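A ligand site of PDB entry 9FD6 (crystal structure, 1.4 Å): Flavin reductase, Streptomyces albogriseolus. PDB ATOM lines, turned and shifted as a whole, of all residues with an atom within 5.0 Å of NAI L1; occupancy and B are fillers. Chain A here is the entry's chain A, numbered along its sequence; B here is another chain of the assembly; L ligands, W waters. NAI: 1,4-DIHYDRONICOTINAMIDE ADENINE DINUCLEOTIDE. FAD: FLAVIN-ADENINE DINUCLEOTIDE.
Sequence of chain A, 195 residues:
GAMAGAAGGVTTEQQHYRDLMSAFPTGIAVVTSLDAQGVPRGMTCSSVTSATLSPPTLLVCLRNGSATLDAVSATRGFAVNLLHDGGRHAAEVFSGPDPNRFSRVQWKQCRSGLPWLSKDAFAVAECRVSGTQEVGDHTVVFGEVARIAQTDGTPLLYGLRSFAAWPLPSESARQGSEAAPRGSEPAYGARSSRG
A ring nitrogen (NE2) of His 138 sits at hydrogen-bond distance from a nitrogen (N7N) of NAI L1 (2.8 Å).
OG of Ser 50 of chain B lies within hydrogen-bond range of N3A of NAI L1 (2.7 Å).
The guanidinium group (NH2) of Arg 161 lies within salt-bridge range of an oxygen (O1A) of NAI L1, at 2.9 Å.
A nitrogen (N3) of FAD L2 lies within hydrogen-bond range of the backbone carbonyl oxygen (O) of Cys 61, at 2.8 Å.
The guanidinium group (NH1) of Arg 18 is in salt-bridge range of an oxygen (O2A) of NAI L1 (3.6 Å).
N of Ser 46 is in hydrogen-bond range of N5 of FAD L2 (3.2 Å).
O2N of NAI L1 sits at hydrogen-bond distance from OH of Tyr 158 (2.6 Å).
The guanidinium group (NH2) of Arg 63 lies within salt-bridge range of an oxygen (O1A) of FAD L2 (2.7 Å).
N of Arg 63 is in hydrogen-bond range of O2 of FAD L2, at 2.9 Å.
N5 of FAD L2 sits at hydrogen-bond distance from OG of Ser 46.
A nitrogen (N1) of FAD L2 is in hydrogen-bond range of a nitrogen (N7N) of NAI L1 (3.3 Å).
NH2 of Arg 18 sits at hydrogen-bond distance from OE1 of Gln 15, at 2.7 Å.
The side-chain sulfur (SG) of Cys 61 sits at hydrogen-bond distance from the backbone carbonyl oxygen (O) of Ala 51 of chain B (3.3 Å).
OG of Ser 50 of chain B lies within hydrogen-bond range of OH of Tyr 17, 2.7 Å away.
The backbone NH (N) of Arg 161 is in hydrogen-bond range of the side-chain hydroxyl (OG) of Ser 22 (3.5 Å).
Met 21 touches NAI L1 (CB to O2B, 3.4 Å).
Ser 22 touches NAI L1.
Ser 46 touches NAI L1 (OG to C5N, 3.7 Å).
Ala 51 of chain B touches NAI L1.
Thr 52 of chain B touches NAI L1 (CA to C2A, 3.9 Å).
CG of Leu 53 of chain B touches C6A of NAI L1, at 3.6 Å.
Hydrophobic or aromatic side chains within 4 Å of NAI L1: Met 21, His 138, Tyr 158 and Leu 53 of chain B.
Water W1 lies within hydrogen-bond range of O of Ser 50 of chain B (2.7 Å) and O7N of NAI L1 (2.7 Å).
Water W2 lies within hydrogen-bond range of the side-chain hydroxyl of Ser 22 (2.6 Å), an oxygen (O1N) of NAI L1 (2.7 Å) and the backbone NH of Arg 161 (3.0 Å).
Water W3 lies within hydrogen-bond range of the side-chain hydroxyl (OG) of Ser 46 and an oxygen (O3B) of NAI L1.
Water W6 lies within hydrogen-bond range of the guanidinium group of Arg 18 (2.7 Å) and a nitrogen (N7A) of NAI L1 (3.0 Å).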
ATOM      1  N   GLN A  15       9.136  28.848   0.793  1.00  0.00           N
ATOM      2  CA  GLN A  15       9.993  28.702  -0.382  1.00  0.00           C
ATOM      3  C   GLN A  15      10.866  27.457  -0.290  1.00  0.00           C
ATOM      4  O   GLN A  15      11.056  26.750  -1.279  1.00  0.00           O
ATOM      5  CB  GLN A  15      10.849  29.958  -0.583  1.00  0.00           C
ATOM      6  CG  GLN A  15      11.719  29.906  -1.838  1.00  0.00           C
ATOM      7  CD  GLN A  15      10.868  29.842  -3.090  1.00  0.00           C
ATOM      8  OE1 GLN A  15       9.987  30.676  -3.278  1.00  0.00           O
ATOM      9  NE2 GLN A  15      11.127  28.861  -3.941  1.00  0.00           N
ATOM     10  N   TYR A  17      10.097  24.793   1.163  1.00  0.00           N
ATOM     11  CA  TYR A  17       9.193  23.672   0.909  1.00  0.00           C
ATOM     12  C   TYR A  17       8.871  23.553  -0.576  1.00  0.00           C
ATOM     13  O   TYR A  17       8.843  22.443  -1.121  1.00  0.00           O
ATOM     14  CB  TYR A  17       7.933  23.843   1.755  1.00  0.00           C
ATOM     15  CG  TYR A  17       6.856  22.867   1.416  1.00  0.00           C
ATOM     16  CD1 TYR A  17       6.890  21.566   1.889  1.00  0.00           C
ATOM     17  CD2 TYR A  17       5.791  23.233   0.595  1.00  0.00           C
ATOM     18  CE1 TYR A  17       5.909  20.670   1.578  1.00  0.00           C
ATOM     19  CE2 TYR A  17       4.798  22.342   0.263  1.00  0.00           C
ATOM     20  CZ  TYR A  17       4.863  21.058   0.765  1.00  0.00           C
ATOM     21  OH  TYR A  17       3.883  20.133   0.466  1.00  0.00           O
ATOM     22  N   ARG A  18       8.645  24.682  -1.258  1.00  0.00           N
ATOM     23  CA  ARG A  18       8.475  24.619  -2.709  1.00  0.00           C
ATOM     24  C   ARG A  18       9.702  24.030  -3.392  1.00  0.00           C
ATOM     25  O   ARG A  18       9.577  23.225  -4.319  1.00  0.00           O
ATOM     26  CB  ARG A  18       8.149  26.003  -3.274  1.00  0.00           C
ATOM     27  CG  ARG A  18       6.810  26.549  -2.779  1.00  0.00           C
ATOM     28  CD  ARG A  18       6.230  27.625  -3.690  1.00  0.00           C
ATOM     29  NE  ARG A  18       7.108  28.765  -3.901  1.00  0.00           N
ATOM     30  CZ  ARG A  18       6.732  29.892  -4.495  1.00  0.00           C
ATOM     31  NH1 ARG A  18       5.478  30.091  -4.873  1.00  0.00           N
ATOM     32  NH2 ARG A  18       7.643  30.850  -4.701  1.00  0.00           N
ATOM     33  N   MET A  21       9.389  20.196  -2.907  1.00  0.00           N
ATOM     34  CA  MET A  21       8.331  19.527  -3.649  1.00  0.00           C
ATOM     35  C   MET A  21       8.540  19.652  -5.153  1.00  0.00           C
ATOM     36  O   MET A  21       8.087  18.798  -5.911  1.00  0.00           O
ATOM     37  CB  MET A  21       6.975  20.073  -3.205  1.00  0.00           C
ATOM     38  CG  MET A  21       6.662  19.847  -1.729  1.00  0.00           C
ATOM     39  SD  MET A  21       6.919  18.151  -1.174  1.00  0.00           S
ATOM     40  CE  MET A  21       5.582  17.323  -1.994  1.00  0.00           C
ATOM     41  N   SER A  22       9.240  20.695  -5.599  1.00  0.00           N
ATOM     42  CA  SER A  22       9.530  20.807  -7.017  1.00  0.00           C
ATOM     43  C   SER A  22      10.340  19.608  -7.515  1.00  0.00           C
ATOM     44  O   SER A  22      10.212  19.205  -8.678  1.00  0.00           O
ATOM     45  CB  SER A  22      10.276  22.107  -7.286  1.00  0.00           C
ATOM     46  OG  SER A  22      10.510  22.258  -8.661  1.00  0.00           O
ATOM     47  N   SER A  46      -1.365  18.516 -10.644  1.00  0.00           N
ATOM     48  CA  SER A  46      -0.262  17.590 -10.464  1.00  0.00           C
ATOM     49  C   SER A  46      -0.427  16.736  -9.210  1.00  0.00           C
ATOM     50  O   SER A  46       0.451  15.923  -8.917  1.00  0.00           O
ATOM     51  CB  SER A  46       1.063  18.363 -10.395  1.00  0.00           C
ATOM     52  OG  SER A  46       1.042  19.319  -9.350  1.00  0.00           O
ATOM     53  N   CYS A  61      -5.828  17.400  -4.938  1.00  0.00           N
ATOM     54  CA  CYS A  61      -5.772  18.475  -3.956  1.00  0.00           C
ATOM     55  C   CYS A  61      -5.978  19.796  -4.684  1.00  0.00           C
ATOM     56  O   CYS A  61      -5.117  20.202  -5.476  1.00  0.00           O
ATOM     57  CB  CYS A  61      -4.446  18.444  -3.198  1.00  0.00           C
ATOM     58  SG  CYS A  61      -4.379  19.609  -1.841  1.00  0.00           S
ATOM     59  N   ARG A  63      -7.171  24.026  -4.741  1.00  0.00           N
ATOM     60  CA  ARG A  63      -7.139  25.255  -3.968  1.00  0.00           C
ATOM     61  C   ARG A  63      -8.538  25.726  -3.580  1.00  0.00           C
ATOM     62  O   ARG A  63      -9.456  25.756  -4.403  1.00  0.00           O
ATOM     63  CB  ARG A  63      -6.446  26.345  -4.794  1.00  0.00           C
ATOM     64  CG  ARG A  63      -6.175  27.617  -4.028  1.00  0.00           C
ATOM     65  CD  ARG A  63      -5.678  28.704  -4.969  1.00  0.00           C
ATOM     66  NE  ARG A  63      -6.788  29.501  -5.462  1.00  0.00           N
ATOM     67  CZ  ARG A  63      -7.129  29.656  -6.749  1.00  0.00           C
ATOM     68  NH1 ARG A  63      -6.411  29.110  -7.718  1.00  0.00           N
ATOM     69  NH2 ARG A  63      -8.186  30.389  -7.047  1.00  0.00           N
ATOM     70  N   HIS A 138      -6.367  24.445   0.976  1.00  0.00           N
ATOM     71  CA  HIS A 138      -6.679  23.477  -0.053  1.00  0.00           C
ATOM     72  C   HIS A 138      -7.691  22.487   0.478  1.00  0.00           C
ATOM     73  O   HIS A 138      -7.952  22.406   1.683  1.00  0.00           O
ATOM     74  CB  HIS A 138      -5.433  22.713  -0.504  1.00  0.00           C
ATOM     75  CG  HIS A 138      -4.626  23.434  -1.524  1.00  0.00           C
ATOM     76  ND1 HIS A 138      -4.031  24.649  -1.284  1.00  0.00           N
ATOM     77  CD2 HIS A 138      -4.322  23.115  -2.799  1.00  0.00           C
ATOM     78  CE1 HIS A 138      -3.397  25.051  -2.362  1.00  0.00           C
ATOM     79  NE2 HIS A 138      -3.552  24.134  -3.298  1.00  0.00           N
ATOM     80  N   TYR A 158       5.935  16.935 -15.343  1.00  0.00           N
ATOM     81  CA  TYR A 158       6.355  18.233 -14.843  1.00  0.00           C
ATOM     82  C   TYR A 158       7.206  17.999 -13.605  1.00  0.00           C
ATOM     83  O   TYR A 158       6.808  17.242 -12.715  1.00  0.00           O
ATOM     84  CB  TYR A 158       5.157  19.108 -14.488  1.00  0.00           C
ATOM     85  CG  TYR A 158       5.513  20.563 -14.279  1.00  0.00           C
ATOM     86  CD1 TYR A 158       5.596  21.429 -15.357  1.00  0.00           C
ATOM     87  CD2 TYR A 158       5.764  21.066 -13.014  1.00  0.00           C
ATOM     88  CE1 TYR A 158       5.908  22.767 -15.174  1.00  0.00           C
ATOM     89  CE2 TYR A 158       6.078  22.408 -12.822  1.00  0.00           C
ATOM     90  CZ  TYR A 158       6.141  23.252 -13.907  1.00  0.00           C
ATOM     91  OH  TYR A 158       6.462  24.591 -13.738  1.00  0.00           O
ATOM     92  N   ARG A 161      10.379  22.573 -12.112  1.00  0.00           N
ATOM     93  CA  ARG A 161       9.878  23.766 -12.781  1.00  0.00           C
ATOM     94  C   ARG A 161       9.955  23.672 -14.308  1.00  0.00           C
ATOM     95  O   ARG A 161      10.104  24.684 -14.984  1.00  0.00           O
ATOM     96  CB  ARG A 161      10.566  25.023 -12.235  1.00  0.00           C
ATOM     97  CG  ARG A 161      10.339  25.151 -10.727  1.00  0.00           C
ATOM     98  CD  ARG A 161      11.154  26.241 -10.050  1.00  0.00           C
ATOM     99  NE  ARG A 161      10.852  26.243  -8.623  1.00  0.00           N
ATOM    100  CZ  ARG A 161      11.738  26.131  -7.641  1.00  0.00           C
ATOM    101  NH1 ARG A 161      13.042  26.154  -7.874  1.00  0.00           N
ATOM    102  NH2 ARG A 161      11.311  26.018  -6.388  1.00  0.00           N
ATOM    103  N   SER B  50       1.809  17.306  -2.464  1.00  0.00           N
ATOM    104  CA  SER B  50       1.753  18.571  -1.739  1.00  0.00           C
ATOM    105  C   SER B  50       0.306  18.897  -1.409  1.00  0.00           C
ATOM    106  O   SER B  50      -0.568  18.816  -2.262  1.00  0.00           O
ATOM    107  CB  SER B  50       2.335  19.690  -2.594  1.00  0.00           C
ATOM    108  OG  SER B  50       2.555  20.834  -1.789  1.00  0.00           O
ATOM    109  N   ALA B  51       0.060  19.299  -0.165  1.00  0.00           N
ATOM    110  CA  ALA B  51      -1.289  19.658   0.259  1.00  0.00           C
ATOM    111  C   ALA B  51      -1.482  21.177   0.331  1.00  0.00           C
ATOM    112  O   ALA B  51      -2.370  21.720  -0.324  1.00  0.00           O
ATOM    113  CB  ALA B  51      -1.618  19.005   1.603  1.00  0.00           C
ATOM    114  N   THR B  52      -0.638  21.865   1.101  1.00  0.00           N
ATOM    115  CA  THR B  52      -0.763  23.309   1.244  1.00  0.00           C
ATOM    116  C   THR B  52       0.581  23.898   1.661  1.00  0.00           C
ATOM    117  O   THR B  52       1.455  23.183   2.160  1.00  0.00           O
ATOM    118  CB  THR B  52      -1.835  23.676   2.278  1.00  0.00           C
ATOM    119  OG1 THR B  52      -1.975  25.101   2.355  1.00  0.00           O
ATOM    120  CG2 THR B  52      -1.446  23.145   3.653  1.00  0.00           C
ATOM    121  N   LEU B  53       0.729  25.204   1.452  1.00  0.00           N
ATOM    122  CA  LEU B  53       1.878  25.934   1.962  1.00  0.00           C
ATOM    123  C   LEU B  53       1.663  26.530   3.346  1.00  0.00           C
ATOM    124  O   LEU B  53       2.651  26.910   3.989  1.00  0.00           O
ATOM    125  CB  LEU B  53       2.258  27.085   1.012  1.00  0.00           C
ATOM    126  CG  LEU B  53       2.555  26.744  -0.442  1.00  0.00           C
ATOM    127  CD1 LEU B  53       2.878  28.031  -1.187  1.00  0.00           C
ATOM    128  CD2 LEU B  53       3.681  25.716  -0.573  1.00  0.00           C
HETATM  129  PA  NAI L   1       7.142  26.429  -7.438  1.00  0.00           P
HETATM  130  O1A NAI L   1       8.532  26.510  -6.919  1.00  0.00           O
HETATM  131  O2A NAI L   1       6.210  27.596  -7.333  1.00  0.00           O
HETATM  132  O5B NAI L   1       6.371  25.181  -6.711  1.00  0.00           O
HETATM  133  C5B NAI L   1       7.092  24.001  -6.470  1.00  0.00           C
HETATM  134  C4B NAI L   1       6.204  22.925  -5.901  1.00  0.00           C
HETATM  135  O4B NAI L   1       5.724  23.315  -4.610  1.00  0.00           O
HETATM  136  C3B NAI L   1       4.947  22.685  -6.713  1.00  0.00           C
HETATM  137  O3B NAI L   1       5.238  21.842  -7.794  1.00  0.00           O
HETATM  138  C2B NAI L   1       4.110  22.008  -5.626  1.00  0.00           C
HETATM  139  O2B NAI L   1       4.476  20.678  -5.423  1.00  0.00           O
HETATM  140  C1B NAI L   1       4.418  22.870  -4.402  1.00  0.00           C
HETATM  141  N9A NAI L   1       3.491  23.979  -4.272  1.00  0.00           N
HETATM  142  C8A NAI L   1       3.644  25.228  -4.807  1.00  0.00           C
HETATM  143  N7A NAI L   1       2.653  26.029  -4.566  1.00  0.00           N
HETATM  144  C5A NAI L   1       1.787  25.293  -3.828  1.00  0.00           C
HETATM  145  C6A NAI L   1       0.543  25.602  -3.264  1.00  0.00           C
HETATM  146  N6A NAI L   1      -0.018  26.803  -3.377  1.00  0.00           N
HETATM  147  N1A NAI L   1      -0.084  24.654  -2.575  1.00  0.00           N
HETATM  148  C2A NAI L   1       0.500  23.464  -2.473  1.00  0.00           C
HETATM  149  N3A NAI L   1       1.662  23.046  -2.955  1.00  0.00           N
HETATM  150  C4A NAI L   1       2.285  24.010  -3.638  1.00  0.00           C
HETATM  151  O3  NAI L   1       7.252  25.921  -8.980  1.00  0.00           O
HETATM  152  PN  NAI L   1       6.300  25.031  -9.970  1.00  0.00           P
HETATM  153  O1N NAI L   1       6.306  23.602  -9.533  1.00  0.00           O
HETATM  154  O2N NAI L   1       6.734  25.444 -11.336  1.00  0.00           O
HETATM  155  O5D NAI L   1       4.775  25.570  -9.679  1.00  0.00           O
HETATM  156  C5D NAI L   1       4.426  26.835 -10.173  1.00  0.00           C
HETATM  157  C4D NAI L   1       3.105  27.276  -9.579  1.00  0.00           C
HETATM  158  O4D NAI L   1       2.013  26.396  -9.878  1.00  0.00           O
HETATM  159  C3D NAI L   1       3.157  27.311  -8.049  1.00  0.00           C
HETATM  160  O3D NAI L   1       3.784  28.498  -7.624  1.00  0.00           O
HETATM  161  C2D NAI L   1       1.646  27.318  -7.761  1.00  0.00           C
HETATM  162  O2D NAI L   1       1.032  28.565  -7.927  1.00  0.00           O
HETATM  163  C1D NAI L   1       1.106  26.345  -8.815  1.00  0.00           C
HETATM  164  N1N NAI L   1       0.932  25.013  -8.293  1.00  0.00           N
HETATM  165  C2N NAI L   1      -0.023  24.751  -7.371  1.00  0.00           C
HETATM  166  C3N NAI L   1      -0.185  23.568  -6.738  1.00  0.00           C
HETATM  167  C7N NAI L   1      -1.256  23.437  -5.741  1.00  0.00           C
HETATM  168  O7N NAI L   1      -1.460  22.401  -5.095  1.00  0.00           O
HETATM  169  N7N NAI L   1      -2.021  24.541  -5.574  1.00  0.00           N
HETATM  170  C4N NAI L   1       0.639  22.364  -7.103  1.00  0.00           C
HETATM  171  C5N NAI L   1       1.705  22.777  -8.078  1.00  0.00           C
HETATM  172  C6N NAI L   1       1.749  23.950  -8.685  1.00  0.00           C
HETATM  173  PA  FAD L   2      -9.301  30.217 -10.415  1.00  0.00           P
HETATM  174  O1A FAD L   2      -8.068  30.771  -9.749  1.00  0.00           O
HETATM  175  O2A FAD L   2     -10.622  30.237  -9.733  1.00  0.00           O
HETATM  176  O5B FAD L   2      -9.480  30.943 -11.856  1.00  0.00           O
HETATM  177  C5B FAD L   2      -8.435  31.212 -12.762  1.00  0.00           C
HETATM  178  C4B FAD L   2      -8.725  32.592 -13.381  1.00  0.00           C
HETATM  179  O4B FAD L   2     -10.089  32.678 -13.813  1.00  0.00           O
HETATM  180  C3B FAD L   2      -8.526  33.736 -12.389  1.00  0.00           C
HETATM  181  O3B FAD L   2      -8.078  34.856 -13.117  1.00  0.00           O
HETATM  182  C2B FAD L   2      -9.934  33.919 -11.847  1.00  0.00           C
HETATM  183  O2B FAD L   2     -10.114  35.196 -11.297  1.00  0.00           O
HETATM  184  C1B FAD L   2     -10.813  33.651 -13.078  1.00  0.00           C
HETATM  185  N9A FAD L   2     -12.143  33.144 -12.802  1.00  0.00           N
HETATM  186  C8A FAD L   2     -12.446  32.078 -12.002  1.00  0.00           C
HETATM  187  N7A FAD L   2     -13.726  31.817 -11.940  1.00  0.00           N
HETATM  188  C5A FAD L   2     -14.308  32.763 -12.747  1.00  0.00           C
HETATM  189  C6A FAD L   2     -15.646  33.011 -13.078  1.00  0.00           C
HETATM  190  N6A FAD L   2     -16.654  32.265 -12.613  1.00  0.00           N
HETATM  191  N1A FAD L   2     -15.888  34.026 -13.920  1.00  0.00           N
HETATM  192  C2A FAD L   2     -14.866  34.748 -14.378  1.00  0.00           C
HETATM  193  N3A FAD L   2     -13.571  34.614 -14.120  1.00  0.00           N
HETATM  194  C4A FAD L   2     -13.341  33.603 -13.300  1.00  0.00           C
HETATM  195  N1  FAD L   2      -3.612  23.897  -8.396  1.00  0.00           N
HETATM  196  C2  FAD L   2      -4.265  23.082  -7.512  1.00  0.00           C
HETATM  197  O2  FAD L   2      -5.177  23.467  -6.801  1.00  0.00           O
HETATM  198  N3  FAD L   2      -3.859  21.756  -7.435  1.00  0.00           N
HETATM  199  C4  FAD L   2      -2.854  21.154  -8.153  1.00  0.00           C
HETATM  200  O4  FAD L   2      -2.559  19.985  -8.037  1.00  0.00           O
HETATM  201  C4X FAD L   2      -2.155  22.060  -9.102  1.00  0.00           C
HETATM  202  N5  FAD L   2      -1.183  21.579  -9.832  1.00  0.00           N
HETATM  203  C5X FAD L   2      -0.544  22.413 -10.709  1.00  0.00           C
HETATM  204  C6  FAD L   2       0.527  21.934 -11.512  1.00  0.00           C
HETATM  205  C7  FAD L   2       1.204  22.726 -12.404  1.00  0.00           C
HETATM  206  C7M FAD L   2       2.333  22.212 -13.241  1.00  0.00           C
HETATM  207  C8  FAD L   2       0.808  24.082 -12.486  1.00  0.00           C
HETATM  208  C8M FAD L   2       1.482  25.035 -13.427  1.00  0.00           C
HETATM  209  C9  FAD L   2      -0.232  24.569 -11.718  1.00  0.00           C
HETATM  210  C9A FAD L   2      -0.942  23.769 -10.814  1.00  0.00           C
HETATM  211  N10 FAD L   2      -1.982  24.247 -10.019  1.00  0.00           N
HETATM  212  C10 FAD L   2      -2.628  23.425  -9.144  1.00  0.00           C
HETATM  213  C1' FAD L   2      -2.464  25.638 -10.126  1.00  0.00           C
HETATM  214  C2' FAD L   2      -3.745  25.657 -11.015  1.00  0.00           C
HETATM  215  O2' FAD L   2      -3.615  24.913 -12.219  1.00  0.00           O
HETATM  216  C3' FAD L   2      -4.157  27.102 -11.403  1.00  0.00           C
HETATM  217  O3' FAD L   2      -4.315  27.828 -10.205  1.00  0.00           O
HETATM  218  C4' FAD L   2      -5.435  27.153 -12.273  1.00  0.00           C
HETATM  219  O4' FAD L   2      -5.395  28.340 -13.054  1.00  0.00           O
HETATM  220  C5' FAD L   2      -6.724  27.097 -11.452  1.00  0.00           C
HETATM  221  O5' FAD L   2      -7.819  27.213 -12.322  1.00  0.00           O
HETATM  222  P   FAD L   2      -9.348  27.513 -11.799  1.00  0.00           P
HETATM  223  O1P FAD L   2     -10.084  28.054 -12.970  1.00  0.00           O
HETATM  224  O2P FAD L   2      -9.872  26.387 -10.969  1.00  0.00           O
HETATM  225  O3P FAD L   2      -8.999  28.643 -10.662  1.00  0.00           O
HETATM  226  O   HOH W   1      -0.764  19.789  -4.770  1.00  0.00           O
HETATM  227  O   HOH W   2       8.331  21.847 -10.104  1.00  0.00           O
HETATM  228  O   HOH W   3       3.578  19.974  -9.346  1.00  0.00           O
HETATM  229  O   HOH W   4       2.669  30.866  -8.155  1.00  0.00           O
HETATM  230  O   HOH W   5       9.575  28.898  -6.379  1.00  0.00           O
HETATM  231  O   HOH W   6       2.962  29.009  -4.701  1.00  0.00           O
HETATM  232  O   HOH W   7      -2.568  28.236  -2.687  1.00  0.00           O
